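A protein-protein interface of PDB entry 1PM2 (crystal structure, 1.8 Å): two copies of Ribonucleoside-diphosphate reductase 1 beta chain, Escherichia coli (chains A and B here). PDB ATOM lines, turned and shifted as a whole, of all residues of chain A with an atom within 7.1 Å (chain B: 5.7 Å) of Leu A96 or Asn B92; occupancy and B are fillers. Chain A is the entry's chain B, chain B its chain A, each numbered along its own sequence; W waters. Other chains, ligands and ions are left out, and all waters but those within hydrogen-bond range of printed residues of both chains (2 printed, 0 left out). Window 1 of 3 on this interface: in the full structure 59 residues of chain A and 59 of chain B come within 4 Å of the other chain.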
ATOM      1  N   TYR A   2      13.214 -10.986  27.813  1.00  0.00           N
ATOM      2  CA  TYR A   2      13.642 -12.341  27.516  1.00  0.00           C
ATOM      3  C   TYR A   2      14.689 -12.341  26.412  1.00  0.00           C
ATOM      4  O   TYR A   2      14.657 -11.496  25.517  1.00  0.00           O
ATOM      5  CB  TYR A   2      12.450 -13.187  27.061  1.00  0.00           C
ATOM      6  CG  TYR A   2      12.844 -14.581  26.620  1.00  0.00           C
ATOM      7  CD1 TYR A   2      13.045 -15.599  27.552  1.00  0.00           C
ATOM      8  CD2 TYR A   2      13.060 -14.870  25.271  1.00  0.00           C
ATOM      9  CE1 TYR A   2      13.454 -16.870  27.150  1.00  0.00           C
ATOM     10  CE2 TYR A   2      13.470 -16.135  24.860  1.00  0.00           C
ATOM     11  CZ  TYR A   2      13.665 -17.129  25.802  1.00  0.00           C
ATOM     12  OH  TYR A   2      14.072 -18.381  25.396  1.00  0.00           O
ATOM     13  N   PHE A  18      13.076 -21.753  37.759  1.00  0.00           N
ATOM     14  CA  PHE A  18      12.400 -20.668  37.053  1.00  0.00           C
ATOM     15  C   PHE A  18      12.831 -19.278  37.511  1.00  0.00           C
ATOM     16  O   PHE A  18      13.317 -19.097  38.631  1.00  0.00           O
ATOM     17  CB  PHE A  18      10.886 -20.769  37.269  1.00  0.00           C
ATOM     18  CG  PHE A  18      10.289 -22.072  36.840  1.00  0.00           C
ATOM     19  CD1 PHE A  18       9.933 -22.285  35.514  1.00  0.00           C
ATOM     20  CD2 PHE A  18      10.056 -23.082  37.769  1.00  0.00           C
ATOM     21  CE1 PHE A  18       9.346 -23.486  35.116  1.00  0.00           C
ATOM     22  CE2 PHE A  18       9.471 -24.285  37.382  1.00  0.00           C
ATOM     23  CZ  PHE A  18       9.114 -24.486  36.052  1.00  0.00           C
ATOM     24  N   PRO A  22      17.985 -16.508  31.749  1.00  0.00           N
ATOM     25  CA  PRO A  22      17.530 -17.373  30.657  1.00  0.00           C
ATOM     26  C   PRO A  22      18.653 -18.339  30.270  1.00  0.00           C
ATOM     27  O   PRO A  22      19.829 -17.977  30.299  1.00  0.00           O
ATOM     28  CB  PRO A  22      17.207 -16.377  29.548  1.00  0.00           C
ATOM     29  CG  PRO A  22      16.684 -15.202  30.320  1.00  0.00           C
ATOM     30  CD  PRO A  22      17.689 -15.093  31.455  1.00  0.00           C
ATOM     31  N   VAL A  23      18.287 -19.564  29.916  1.00  0.00           N
ATOM     32  CA  VAL A  23      19.273 -20.579  29.545  1.00  0.00           C
ATOM     33  C   VAL A  23      20.029 -20.227  28.266  1.00  0.00           C
ATOM     34  O   VAL A  23      19.408 -19.951  27.238  1.00  0.00           O
ATOM     35  CB  VAL A  23      18.593 -21.957  29.327  1.00  0.00           C
ATOM     36  CG1 VAL A  23      19.637 -23.010  28.976  1.00  0.00           C
ATOM     37  CG2 VAL A  23      17.816 -22.358  30.573  1.00  0.00           C
ATOM     38  N   GLY A  88       0.078 -29.856  23.709  1.00  0.00           N
ATOM     39  CA  GLY A  88       1.114 -29.865  22.696  1.00  0.00           C
ATOM     40  C   GLY A  88       1.812 -28.523  22.573  1.00  0.00           C
ATOM     41  O   GLY A  88       3.016 -28.469  22.319  1.00  0.00           O
ATOM     42  N   SER A  90       1.021 -25.536  24.939  1.00  0.00           N
ATOM     43  CA  SER A  90       1.109 -24.807  26.194  1.00  0.00           C
ATOM     44  C   SER A  90       2.360 -24.897  27.062  1.00  0.00           C
ATOM     45  O   SER A  90       2.834 -23.875  27.552  1.00  0.00           O
ATOM     46  CB  SER A  90      -0.144 -25.101  27.021  1.00  0.00           C
ATOM     47  OG  SER A  90      -1.298 -24.762  26.259  1.00  0.00           O
ATOM     48  N   PRO A  91       2.908 -26.102  27.281  1.00  0.00           N
ATOM     49  CA  PRO A  91       4.114 -26.122  28.116  1.00  0.00           C
ATOM     50  C   PRO A  91       5.220 -25.257  27.499  1.00  0.00           C
ATOM     51  O   PRO A  91       5.943 -24.557  28.208  1.00  0.00           O
ATOM     52  CB  PRO A  91       4.477 -27.602  28.157  1.00  0.00           C
ATOM     53  CG  PRO A  91       3.124 -28.270  28.115  1.00  0.00           C
ATOM     54  CD  PRO A  91       2.407 -27.468  27.039  1.00  0.00           C
ATOM     55  N   ASN A  92       5.337 -25.295  26.174  1.00  0.00           N
ATOM     56  CA  ASN A  92       6.351 -24.502  25.483  1.00  0.00           C
ATOM     57  C   ASN A  92       6.095 -23.002  25.595  1.00  0.00           C
ATOM     58  O   ASN A  92       6.971 -22.243  26.008  1.00  0.00           O
ATOM     59  CB  ASN A  92       6.423 -24.867  23.996  1.00  0.00           C
ATOM     60  CG  ASN A  92       7.201 -26.145  23.737  1.00  0.00           C
ATOM     61  OD1 ASN A  92       8.142 -26.472  24.458  1.00  0.00           O
ATOM     62  ND2 ASN A  92       6.829 -26.859  22.681  1.00  0.00           N
ATOM     63  N   VAL A  93       4.891 -22.575  25.233  1.00  0.00           N
ATOM     64  CA  VAL A  93       4.565 -21.152  25.268  1.00  0.00           C
ATOM     65  C   VAL A  93       4.585 -20.558  26.670  1.00  0.00           C
ATOM     66  O   VAL A  93       5.069 -19.444  26.867  1.00  0.00           O
ATOM     67  CB  VAL A  93       3.181 -20.880  24.627  1.00  0.00           C
ATOM     68  CG1 VAL A  93       2.848 -19.390  24.707  1.00  0.00           C
ATOM     69  CG2 VAL A  93       3.190 -21.328  23.173  1.00  0.00           C
ATOM     70  N   ALA A  94       4.083 -21.312  27.644  1.00  0.00           N
ATOM     71  CA  ALA A  94       4.014 -20.836  29.021  1.00  0.00           C
ATOM     72  C   ALA A  94       5.282 -20.979  29.860  1.00  0.00           C
ATOM     73  O   ALA A  94       5.597 -20.099  30.665  1.00  0.00           O
ATOM     74  CB  ALA A  94       2.848 -21.523  29.740  1.00  0.00           C
ATOM     75  N   LEU A  95       6.017 -22.070  29.679  1.00  0.00           N
ATOM     76  CA  LEU A  95       7.208 -22.300  30.494  1.00  0.00           C
ATOM     77  C   LEU A  95       8.567 -21.912  29.922  1.00  0.00           C
ATOM     78  O   LEU A  95       9.446 -21.479  30.665  1.00  0.00           O
ATOM     79  CB  LEU A  95       7.240 -23.766  30.937  1.00  0.00           C
ATOM     80  CG  LEU A  95       5.961 -24.253  31.629  1.00  0.00           C
ATOM     81  CD1 LEU A  95       6.090 -25.731  31.977  1.00  0.00           C
ATOM     82  CD2 LEU A  95       5.706 -23.427  32.888  1.00  0.00           C
ATOM     83  N   LEU A  96       8.755 -22.055  28.615  1.00  0.00           N
ATOM     84  CA  LEU A  96      10.044 -21.723  28.023  1.00  0.00           C
ATOM     85  C   LEU A  96      10.588 -20.331  28.362  1.00  0.00           C
ATOM     86  O   LEU A  96      11.782 -20.173  28.619  1.00  0.00           O
ATOM     87  CB  LEU A  96       9.985 -21.916  26.502  1.00  0.00           C
ATOM     88  CG  LEU A  96      10.626 -23.192  25.946  1.00  0.00           C
ATOM     89  CD1 LEU A  96      10.369 -24.369  26.863  1.00  0.00           C
ATOM     90  CD2 LEU A  96      10.102 -23.457  24.539  1.00  0.00           C
ATOM     91  N   PRO A  97       9.724 -19.304  28.381  1.00  0.00           N
ATOM     92  CA  PRO A  97      10.197 -17.952  28.699  1.00  0.00           C
ATOM     93  C   PRO A  97      10.573 -17.747  30.165  1.00  0.00           C
ATOM     94  O   PRO A  97      11.093 -16.692  30.533  1.00  0.00           O
ATOM     95  CB  PRO A  97       9.014 -17.064  28.294  1.00  0.00           C
ATOM     96  CG  PRO A  97       8.304 -17.876  27.255  1.00  0.00           C
ATOM     97  CD  PRO A  97       8.354 -19.261  27.845  1.00  0.00           C
ATOM     98  N   LEU A  98      10.317 -18.751  31.000  1.00  0.00           N
ATOM     99  CA  LEU A  98      10.600 -18.633  32.428  1.00  0.00           C
ATOM    100  C   LEU A  98      11.646 -19.595  32.990  1.00  0.00           C
ATOM    101  O   LEU A  98      12.057 -19.453  34.139  1.00  0.00           O
ATOM    102  CB  LEU A  98       9.306 -18.821  33.223  1.00  0.00           C
ATOM    103  CG  LEU A  98       8.145 -17.859  32.963  1.00  0.00           C
ATOM    104  CD1 LEU A  98       6.905 -18.346  33.703  1.00  0.00           C
ATOM    105  CD2 LEU A  98       8.528 -16.459  33.409  1.00  0.00           C
ATOM    106  N   ILE A  99      12.077 -20.566  32.194  1.00  0.00           N
ATOM    107  CA  ILE A  99      13.045 -21.556  32.665  1.00  0.00           C
ATOM    108  C   ILE A  99      14.487 -21.056  32.677  1.00  0.00           C
ATOM    109  O   ILE A  99      14.921 -20.349  31.764  1.00  0.00           O
ATOM    110  CB  ILE A  99      12.929 -22.847  31.824  1.00  0.00           C
ATOM    111  CG1 ILE A  99      11.545 -23.466  32.054  1.00  0.00           C
ATOM    112  CG2 ILE A  99      14.027 -23.839  32.208  1.00  0.00           C
ATOM    113  CD1 ILE A  99      11.213 -24.628  31.139  1.00  0.00           C
ATOM    114  N   SER A 100      15.226 -21.419  33.725  1.00  0.00           N
ATOM    115  CA  SER A 100      16.614 -20.993  33.854  1.00  0.00           C
ATOM    116  C   SER A 100      17.661 -22.101  34.013  1.00  0.00           C
ATOM    117  O   SER A 100      18.813 -21.816  34.323  1.00  0.00           O
ATOM    118  CB  SER A 100      16.747 -19.965  34.989  1.00  0.00           C
ATOM    119  OG  SER A 100      15.871 -20.246  36.067  1.00  0.00           O
ATOM    120  N   LEU A 104      15.658 -28.682  32.453  1.00  0.00           N
ATOM    121  CA  LEU A 104      14.224 -28.423  32.535  1.00  0.00           C
ATOM    122  C   LEU A 104      13.704 -27.861  31.216  1.00  0.00           C
ATOM    123  O   LEU A 104      12.618 -28.228  30.758  1.00  0.00           O
ATOM    124  CB  LEU A 104      13.925 -27.447  33.676  1.00  0.00           C
ATOM    125  CG  LEU A 104      12.447 -27.119  33.915  1.00  0.00           C
ATOM    126  CD1 LEU A 104      11.644 -28.399  34.109  1.00  0.00           C
ATOM    127  CD2 LEU A 104      12.329 -26.233  35.144  1.00  0.00           C
ATOM    128  N   GLU A 105      14.484 -26.982  30.595  1.00  0.00           N
ATOM    129  CA  GLU A 105      14.071 -26.395  29.328  1.00  0.00           C
ATOM    130  C   GLU A 105      13.867 -27.474  28.271  1.00  0.00           C
ATOM    131  O   GLU A 105      12.845 -27.501  27.587  1.00  0.00           O
ATOM    132  CB  GLU A 105      15.112 -25.388  28.821  1.00  0.00           C
ATOM    133  CG  GLU A 105      14.727 -24.756  27.490  1.00  0.00           C
ATOM    134  CD  GLU A 105      15.815 -23.878  26.911  1.00  0.00           C
ATOM    135  OE1 GLU A 105      16.892 -24.411  26.569  1.00  0.00           O
ATOM    136  OE2 GLU A 105      15.591 -22.654  26.799  1.00  0.00           O
ATOM    137  N   THR A 106      14.843 -28.365  28.128  1.00  0.00           N
ATOM    138  CA  THR A 106      14.727 -29.423  27.137  1.00  0.00           C
ATOM    139  C   THR A 106      13.648 -30.426  27.519  1.00  0.00           C
ATOM    140  O   THR A 106      12.966 -30.964  26.647  1.00  0.00           O
ATOM    141  CB  THR A 106      16.081 -30.134  26.925  1.00  0.00           C
ATOM    142  OG1 THR A 106      17.019 -29.192  26.390  1.00  0.00           O
ATOM    143  CG2 THR A 106      15.941 -31.292  25.943  1.00  0.00           C
ATOM    144  N   TRP A 107      13.468 -30.679  28.812  1.00  0.00           N
ATOM    145  CA  TRP A 107      12.424 -31.619  29.194  1.00  0.00           C
ATOM    146  C   TRP A 107      11.068 -31.081  28.746  1.00  0.00           C
ATOM    147  O   TRP A 107      10.252 -31.814  28.195  1.00  0.00           O
ATOM    148  CB  TRP A 107      12.396 -31.859  30.707  1.00  0.00           C
ATOM    149  CG  TRP A 107      11.148 -32.599  31.130  1.00  0.00           C
ATOM    150  CD1 TRP A 107      10.213 -32.180  32.032  1.00  0.00           C
ATOM    151  CD2 TRP A 107      10.663 -33.842  30.599  1.00  0.00           C
ATOM    152  NE1 TRP A 107       9.171 -33.077  32.089  1.00  0.00           N
ATOM    153  CE2 TRP A 107       9.422 -34.106  31.221  1.00  0.00           C
ATOM    154  CE3 TRP A 107      11.155 -34.754  29.654  1.00  0.00           C
ATOM    155  CZ2 TRP A 107       8.661 -35.248  30.928  1.00  0.00           C
ATOM    156  CZ3 TRP A 107      10.398 -35.892  29.361  1.00  0.00           C
ATOM    157  CH2 TRP A 107       9.163 -36.125  29.999  1.00  0.00           C
ATOM    158  N   VAL A 108      10.832 -29.795  28.978  1.00  0.00           N
ATOM    159  CA  VAL A 108       9.562 -29.192  28.596  1.00  0.00           C
ATOM    160  C   VAL A 108       9.320 -29.315  27.094  1.00  0.00           C
ATOM    161  O   VAL A 108       8.208 -29.624  26.666  1.00  0.00           O
ATOM    162  CB  VAL A 108       9.495 -27.704  29.020  1.00  0.00           C
ATOM    163  CG1 VAL A 108       8.313 -27.015  28.347  1.00  0.00           C
ATOM    164  CG2 VAL A 108       9.350 -27.612  30.533  1.00  0.00           C
ATOM    165  N   GLU A 109      10.355 -29.081  26.295  1.00  0.00           N
ATOM    166  CA  GLU A 109      10.207 -29.183  24.846  1.00  0.00           C
ATOM    167  C   GLU A 109       9.967 -30.632  24.422  1.00  0.00           C
ATOM    168  O   GLU A 109       9.218 -30.898  23.482  1.00  0.00           O
ATOM    169  CB  GLU A 109      11.446 -28.617  24.148  1.00  0.00           C
ATOM    170  CG  GLU A 109      11.750 -27.184  24.551  1.00  0.00           C
ATOM    171  CD  GLU A 109      12.708 -26.502  23.605  1.00  0.00           C
ATOM    172  OE1 GLU A 109      12.279 -26.145  22.486  1.00  0.00           O
ATOM    173  OE2 GLU A 109      13.888 -26.329  23.974  1.00  0.00           O
ATOM    174  N   ALA A 112       6.365 -31.490  25.563  1.00  0.00           N
ATOM    175  CA  ALA A 112       5.429 -30.899  24.608  1.00  0.00           C
ATOM    176  C   ALA A 112       5.434 -31.683  23.296  1.00  0.00           C
ATOM    177  O   ALA A 112       4.385 -31.961  22.722  1.00  0.00           O
ATOM    178  CB  ALA A 112       5.798 -29.445  24.345  1.00  0.00           C
ATOM    179  N   HIS A 168       8.516  -9.479  31.476  1.00  0.00           N
ATOM    180  CA  HIS A 168       9.654  -9.341  30.572  1.00  0.00           C
ATOM    181  C   HIS A 168       9.744  -7.950  29.954  1.00  0.00           C
ATOM    182  O   HIS A 168      10.835  -7.411  29.788  1.00  0.00           O
ATOM    183  CB  HIS A 168       9.599 -10.388  29.452  1.00  0.00           C
ATOM    184  CG  HIS A 168      10.080 -11.745  29.865  1.00  0.00           C
ATOM    185  ND1 HIS A 168      11.259 -11.937  30.555  1.00  0.00           N
ATOM    186  CD2 HIS A 168       9.557 -12.978  29.664  1.00  0.00           C
ATOM    187  CE1 HIS A 168      11.440 -13.230  30.762  1.00  0.00           C
ATOM    188  NE2 HIS A 168      10.422 -13.882  30.230  1.00  0.00           N
ATOM    189  N   GLY B  88      17.171 -24.746  19.387  1.00  0.00           N
ATOM    190  CA  GLY B  88      16.349 -25.665  20.146  1.00  0.00           C
ATOM    191  C   GLY B  88      15.188 -24.934  20.797  1.00  0.00           C
ATOM    192  O   GLY B  88      14.077 -25.459  20.873  1.00  0.00           O
ATOM    193  N   ARG B  89      15.428 -23.708  21.247  1.00  0.00           N
ATOM    194  CA  ARG B  89      14.384 -22.938  21.922  1.00  0.00           C
ATOM    195  C   ARG B  89      13.691 -21.849  21.106  1.00  0.00           C
ATOM    196  O   ARG B  89      12.490 -21.630  21.255  1.00  0.00           O
ATOM    197  CB  ARG B  89      14.960 -22.289  23.188  1.00  0.00           C
ATOM    198  CG  ARG B  89      15.962 -21.160  22.908  1.00  0.00           C
ATOM    199  CD  ARG B  89      16.524 -20.576  24.202  1.00  0.00           C
ATOM    200  NE  ARG B  89      17.278 -21.572  24.960  1.00  0.00           N
ATOM    201  CZ  ARG B  89      18.599 -21.721  24.918  1.00  0.00           C
ATOM    202  NH1 ARG B  89      19.344 -20.927  24.159  1.00  0.00           N
ATOM    203  NH2 ARG B  89      19.177 -22.689  25.622  1.00  0.00           N
ATOM    204  N   SER B  90      14.436 -21.185  20.230  1.00  0.00           N
ATOM    205  CA  SER B  90      13.898 -20.060  19.475  1.00  0.00           C
ATOM    206  C   SER B  90      12.687 -20.261  18.569  1.00  0.00           C
ATOM    207  O   SER B  90      11.760 -19.441  18.593  1.00  0.00           O
ATOM    208  CB  SER B  90      15.039 -19.381  18.719  1.00  0.00           C
ATOM    209  OG  SER B  90      16.010 -18.939  19.658  1.00  0.00           O
ATOM    210  N   PRO B  91      12.669 -21.324  17.748  1.00  0.00           N
ATOM    211  CA  PRO B  91      11.493 -21.507  16.893  1.00  0.00           C
ATOM    212  C   PRO B  91      10.210 -21.537  17.733  1.00  0.00           C
ATOM    213  O   PRO B  91       9.198 -20.930  17.369  1.00  0.00           O
ATOM    214  CB  PRO B  91      11.777 -22.841  16.209  1.00  0.00           C
ATOM    215  CG  PRO B  91      13.273 -22.779  16.018  1.00  0.00           C
ATOM    216  CD  PRO B  91      13.749 -22.255  17.369  1.00  0.00           C
ATOM    217  N   ASN B  92      10.264 -22.237  18.861  1.00  0.00           N
ATOM    218  CA  ASN B  92       9.108 -22.334  19.744  1.00  0.00           C
ATOM    219  C   ASN B  92       8.740 -20.996  20.367  1.00  0.00           C
ATOM    220  O   ASN B  92       7.607 -20.532  20.237  1.00  0.00           O
ATOM    221  CB  ASN B  92       9.356 -23.347  20.866  1.00  0.00           C
ATOM    222  CG  ASN B  92       9.206 -24.779  20.402  1.00  0.00           C
ATOM    223  OD1 ASN B  92       8.424 -25.068  19.498  1.00  0.00           O
ATOM    224  ND2 ASN B  92       9.941 -25.690  21.034  1.00  0.00           N
ATOM    225  N   VAL B  93       9.697 -20.372  21.039  1.00  0.00           N
ATOM    226  CA  VAL B  93       9.433 -19.100  21.697  1.00  0.00           C
ATOM    227  C   VAL B  93       9.029 -17.976  20.748  1.00  0.00           C
ATOM    228  O   VAL B  93       8.105 -17.213  21.038  1.00  0.00           O
ATOM    229  CB  VAL B  93      10.660 -18.635  22.513  1.00  0.00           C
ATOM    230  CG1 VAL B  93      10.349 -17.316  23.202  1.00  0.00           C
ATOM    231  CG2 VAL B  93      11.028 -19.692  23.547  1.00  0.00           C
ATOM    232  N   ALA B  94       9.706 -17.880  19.610  1.00  0.00           N
ATOM    233  CA  ALA B  94       9.425 -16.815  18.659  1.00  0.00           C
ATOM    234  C   ALA B  94       8.276 -17.051  17.676  1.00  0.00           C
ATOM    235  O   ALA B  94       7.562 -16.108  17.327  1.00  0.00           O
ATOM    236  CB  ALA B  94      10.705 -16.473  17.888  1.00  0.00           C
ATOM    237  N   LEU B  95       8.075 -18.293  17.243  1.00  0.00           N
ATOM    238  CA  LEU B  95       7.021 -18.570  16.270  1.00  0.00           C
ATOM    239  C   LEU B  95       5.693 -19.109  16.800  1.00  0.00           C
ATOM    240  O   LEU B  95       4.636 -18.730  16.303  1.00  0.00           O
ATOM    241  CB  LEU B  95       7.556 -19.512  15.182  1.00  0.00           C
ATOM    242  CG  LEU B  95       8.874 -19.098  14.518  1.00  0.00           C
ATOM    243  CD1 LEU B  95       9.266 -20.150  13.486  1.00  0.00           C
ATOM    244  CD2 LEU B  95       8.730 -17.727  13.863  1.00  0.00           C
ATOM    245  N   LEU B  96       5.729 -19.984  17.801  1.00  0.00           N
ATOM    246  CA  LEU B  96       4.488 -20.547  18.334  1.00  0.00           C
ATOM    247  C   LEU B  96       3.376 -19.537  18.606  1.00  0.00           C
ATOM    248  O   LEU B  96       2.231 -19.754  18.209  1.00  0.00           O
ATOM    249  CB  LEU B  96       4.758 -21.356  19.608  1.00  0.00           C
ATOM    250  CG  LEU B  96       5.040 -22.844  19.397  1.00  0.00           C
ATOM    251  CD1 LEU B  96       6.161 -23.014  18.393  1.00  0.00           C
ATOM    252  CD2 LEU B  96       5.397 -23.499  20.721  1.00  0.00           C
ATOM    253  N   PRO B  97       3.692 -18.420  19.283  1.00  0.00           N
ATOM    254  CA  PRO B  97       2.661 -17.420  19.575  1.00  0.00           C
ATOM    255  C   PRO B  97       2.072 -16.719  18.351  1.00  0.00           C
ATOM    256  O   PRO B  97       1.086 -15.991  18.471  1.00  0.00           O
ATOM    257  CB  PRO B  97       3.385 -16.430  20.491  1.00  0.00           C
ATOM    258  CG  PRO B  97       4.463 -17.264  21.129  1.00  0.00           C
ATOM    259  CD  PRO B  97       4.952 -18.080  19.967  1.00  0.00           C
ATOM    260  N   VAL B 108       6.786 -26.614  13.561  1.00  0.00           N
ATOM    261  CA  VAL B 108       7.737 -25.815  14.323  1.00  0.00           C
ATOM    262  C   VAL B 108       8.162 -26.533  15.599  1.00  0.00           C
ATOM    263  O   VAL B 108       9.343 -26.564  15.937  1.00  0.00           O
ATOM    264  CB  VAL B 108       7.152 -24.431  14.682  1.00  0.00           C
ATOM    265  CG1 VAL B 108       8.011 -23.749  15.745  1.00  0.00           C
ATOM    266  CG2 VAL B 108       7.082 -23.572  13.429  1.00  0.00           C
ATOM    267  N   GLU B 109       7.203 -27.121  16.303  1.00  0.00           N
ATOM    268  CA  GLU B 109       7.527 -27.825  17.530  1.00  0.00           C
ATOM    269  C   GLU B 109       8.384 -29.061  17.275  1.00  0.00           C
ATOM    270  O   GLU B 109       9.234 -29.411  18.093  1.00  0.00           O
ATOM    271  CB  GLU B 109       6.241 -28.198  18.270  1.00  0.00           C
ATOM    272  CG  GLU B 109       5.515 -26.971  18.796  1.00  0.00           C
ATOM    273  CD  GLU B 109       4.377 -27.308  19.720  1.00  0.00           C
ATOM    274  OE1 GLU B 109       3.260 -27.564  19.225  1.00  0.00           O
ATOM    275  OE2 GLU B 109       4.610 -27.325  20.947  1.00  0.00           O
ATOM    276  N   ALA B 112      11.901 -27.732  16.257  1.00  0.00           N
ATOM    277  CA  ALA B 112      12.606 -27.312  17.466  1.00  0.00           C
ATOM    278  C   ALA B 112      13.070 -28.525  18.262  1.00  0.00           C
ATOM    279  O   ALA B 112      14.190 -28.553  18.765  1.00  0.00           O
ATOM    280  CB  ALA B 112      11.704 -26.443  18.327  1.00  0.00           C
ATOM    281  N   PHE B 113      12.199 -29.523  18.381  1.00  0.00           N
ATOM    282  CA  PHE B 113      12.545 -30.738  19.105  1.00  0.00           C
ATOM    283  C   PHE B 113      13.784 -31.396  18.497  1.00  0.00           C
ATOM    284  O   PHE B 113      14.707 -31.782  19.216  1.00  0.00           O
ATOM    285  CB  PHE B 113      11.380 -31.731  19.075  1.00  0.00           C
ATOM    286  CG  PHE B 113      11.748 -33.107  19.565  1.00  0.00           C
ATOM    287  CD1 PHE B 113      12.055 -33.323  20.906  1.00  0.00           C
ATOM    288  CD2 PHE B 113      11.819 -34.177  18.679  1.00  0.00           C
ATOM    289  CE1 PHE B 113      12.430 -34.588  21.359  1.00  0.00           C
ATOM    290  CE2 PHE B 113      12.195 -35.449  19.120  1.00  0.00           C
ATOM    291  CZ  PHE B 113      12.500 -35.653  20.464  1.00  0.00           C
HETATM  292  O   HOH W   1       8.892 -28.903  21.037  1.00  0.00           O
HETATM  293  O   HOH W   2       7.235 -21.559  23.143  1.00  0.00           O
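Among the printed residues, merely in contact across the chains: Tyr A2 with Arg B89, Tyr A2 with Val B93, Asn A92 with Asn B92, Asn A92 with Leu B96, Val A93 with Leu B96, Leu A96 with Asn B92, Leu A96 with Val B93 and Glu A109 with Arg B89.
The backbone NH (N) of Tyr A2 lies within hydrogen-bond range of a ring nitrogen (ND1) of His A168, at 3.5 Å.
Leu A96 touches just these residues of chain B: Asn B92 (3.7 Å) and Val B93 (3.8 Å).
Asn B92 touches just these residues of chain A: Asn A92, Leu A96 and Glu A109.
Of the printed residues of chain A, Arg B89 touches Tyr A2, Val A23, Glu A105 and Glu A109.
Of the printed residues of chain A, Val B93 touches Tyr A2 (3.7 Å) and Leu A96 (3.8 Å).
Printed residues of chain B within 4 Å of Glu A109: Gly B88, Arg B89 and Asn B92.
Ser A100 touches none of the printed residues of chain B.
The nearest residue of chain B that does not touch Leu A96 is Arg B89 (4.5 Å).
The nearest residue of chain A that does not touch Asn B92 is Val A93 (5.4 Å).
Water W2 lies within hydrogen-bond range of O of Asn A92 (3.0 Å), O of Asn B92 (3.1 Å), N of Val A93 (3.3 Å) and N of Val B93 (3.4 Å).
Water W1 lies within hydrogen-bond range of the backbone carbonyl oxygen (O) of Glu B109, the backbone carbonyl oxygen (O) of Glu A109, the side-chain amide nitrogen (ND2) of Asn A92 and the side-chain amide nitrogen (ND2) of Asn B92.
The backbone carbonyl oxygen of Gly B88 lies close to the side-chain carboxylate of Glu A109, at 2.5 Å.
NH2 of Arg B89 lies close to O of Val A23 (3.2 Å).
The guanidinium group (NE) of Arg B89 lies within salt-bridge range of the side-chain carboxylate (OE2) of Glu A105 (2.7 Å).
The side-chain amide nitrogen (ND2) of Asn B92 is in hydrogen-bond range of the side-chain carboxylate (OE1) of Glu A109, 2.8 Å away.
The side-chain carboxylate (OE2) of Glu B109 lies within hydrogen-bond range of the side-chain amide nitrogen (ND2) of Asn A92, at 2.9 Å.
O of Gly A88 lies close to OE2 of Glu B109.
Of the 14 printed residues of chain B, 6 touch a printed residue of chain A.
Along chain B the printed residues that touch a printed residue of chain A span positions 88 to 109.
Hydrophobic or aromatic side chains of chain A that line the printed part of chain B: Tyr A2, Val A23, Val A93 and Leu A96.
Gly A88 touches Glu B109, and with the chains exchanged Glu A109 touches Gly B88.
Asn B92 touches its own counterpart, Asn A92.
Asn A92 touches Leu B96, and with the chains exchanged Leu A96 touches Asn B92.
Val A93 touches Leu B96, and with the chains exchanged Leu A96 touches Val B93.
12 positions are printed for both chains.
Of the 14 pairs that touch across the chains among the printed residues, 9 have their exchanged pair printed and touching as well.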
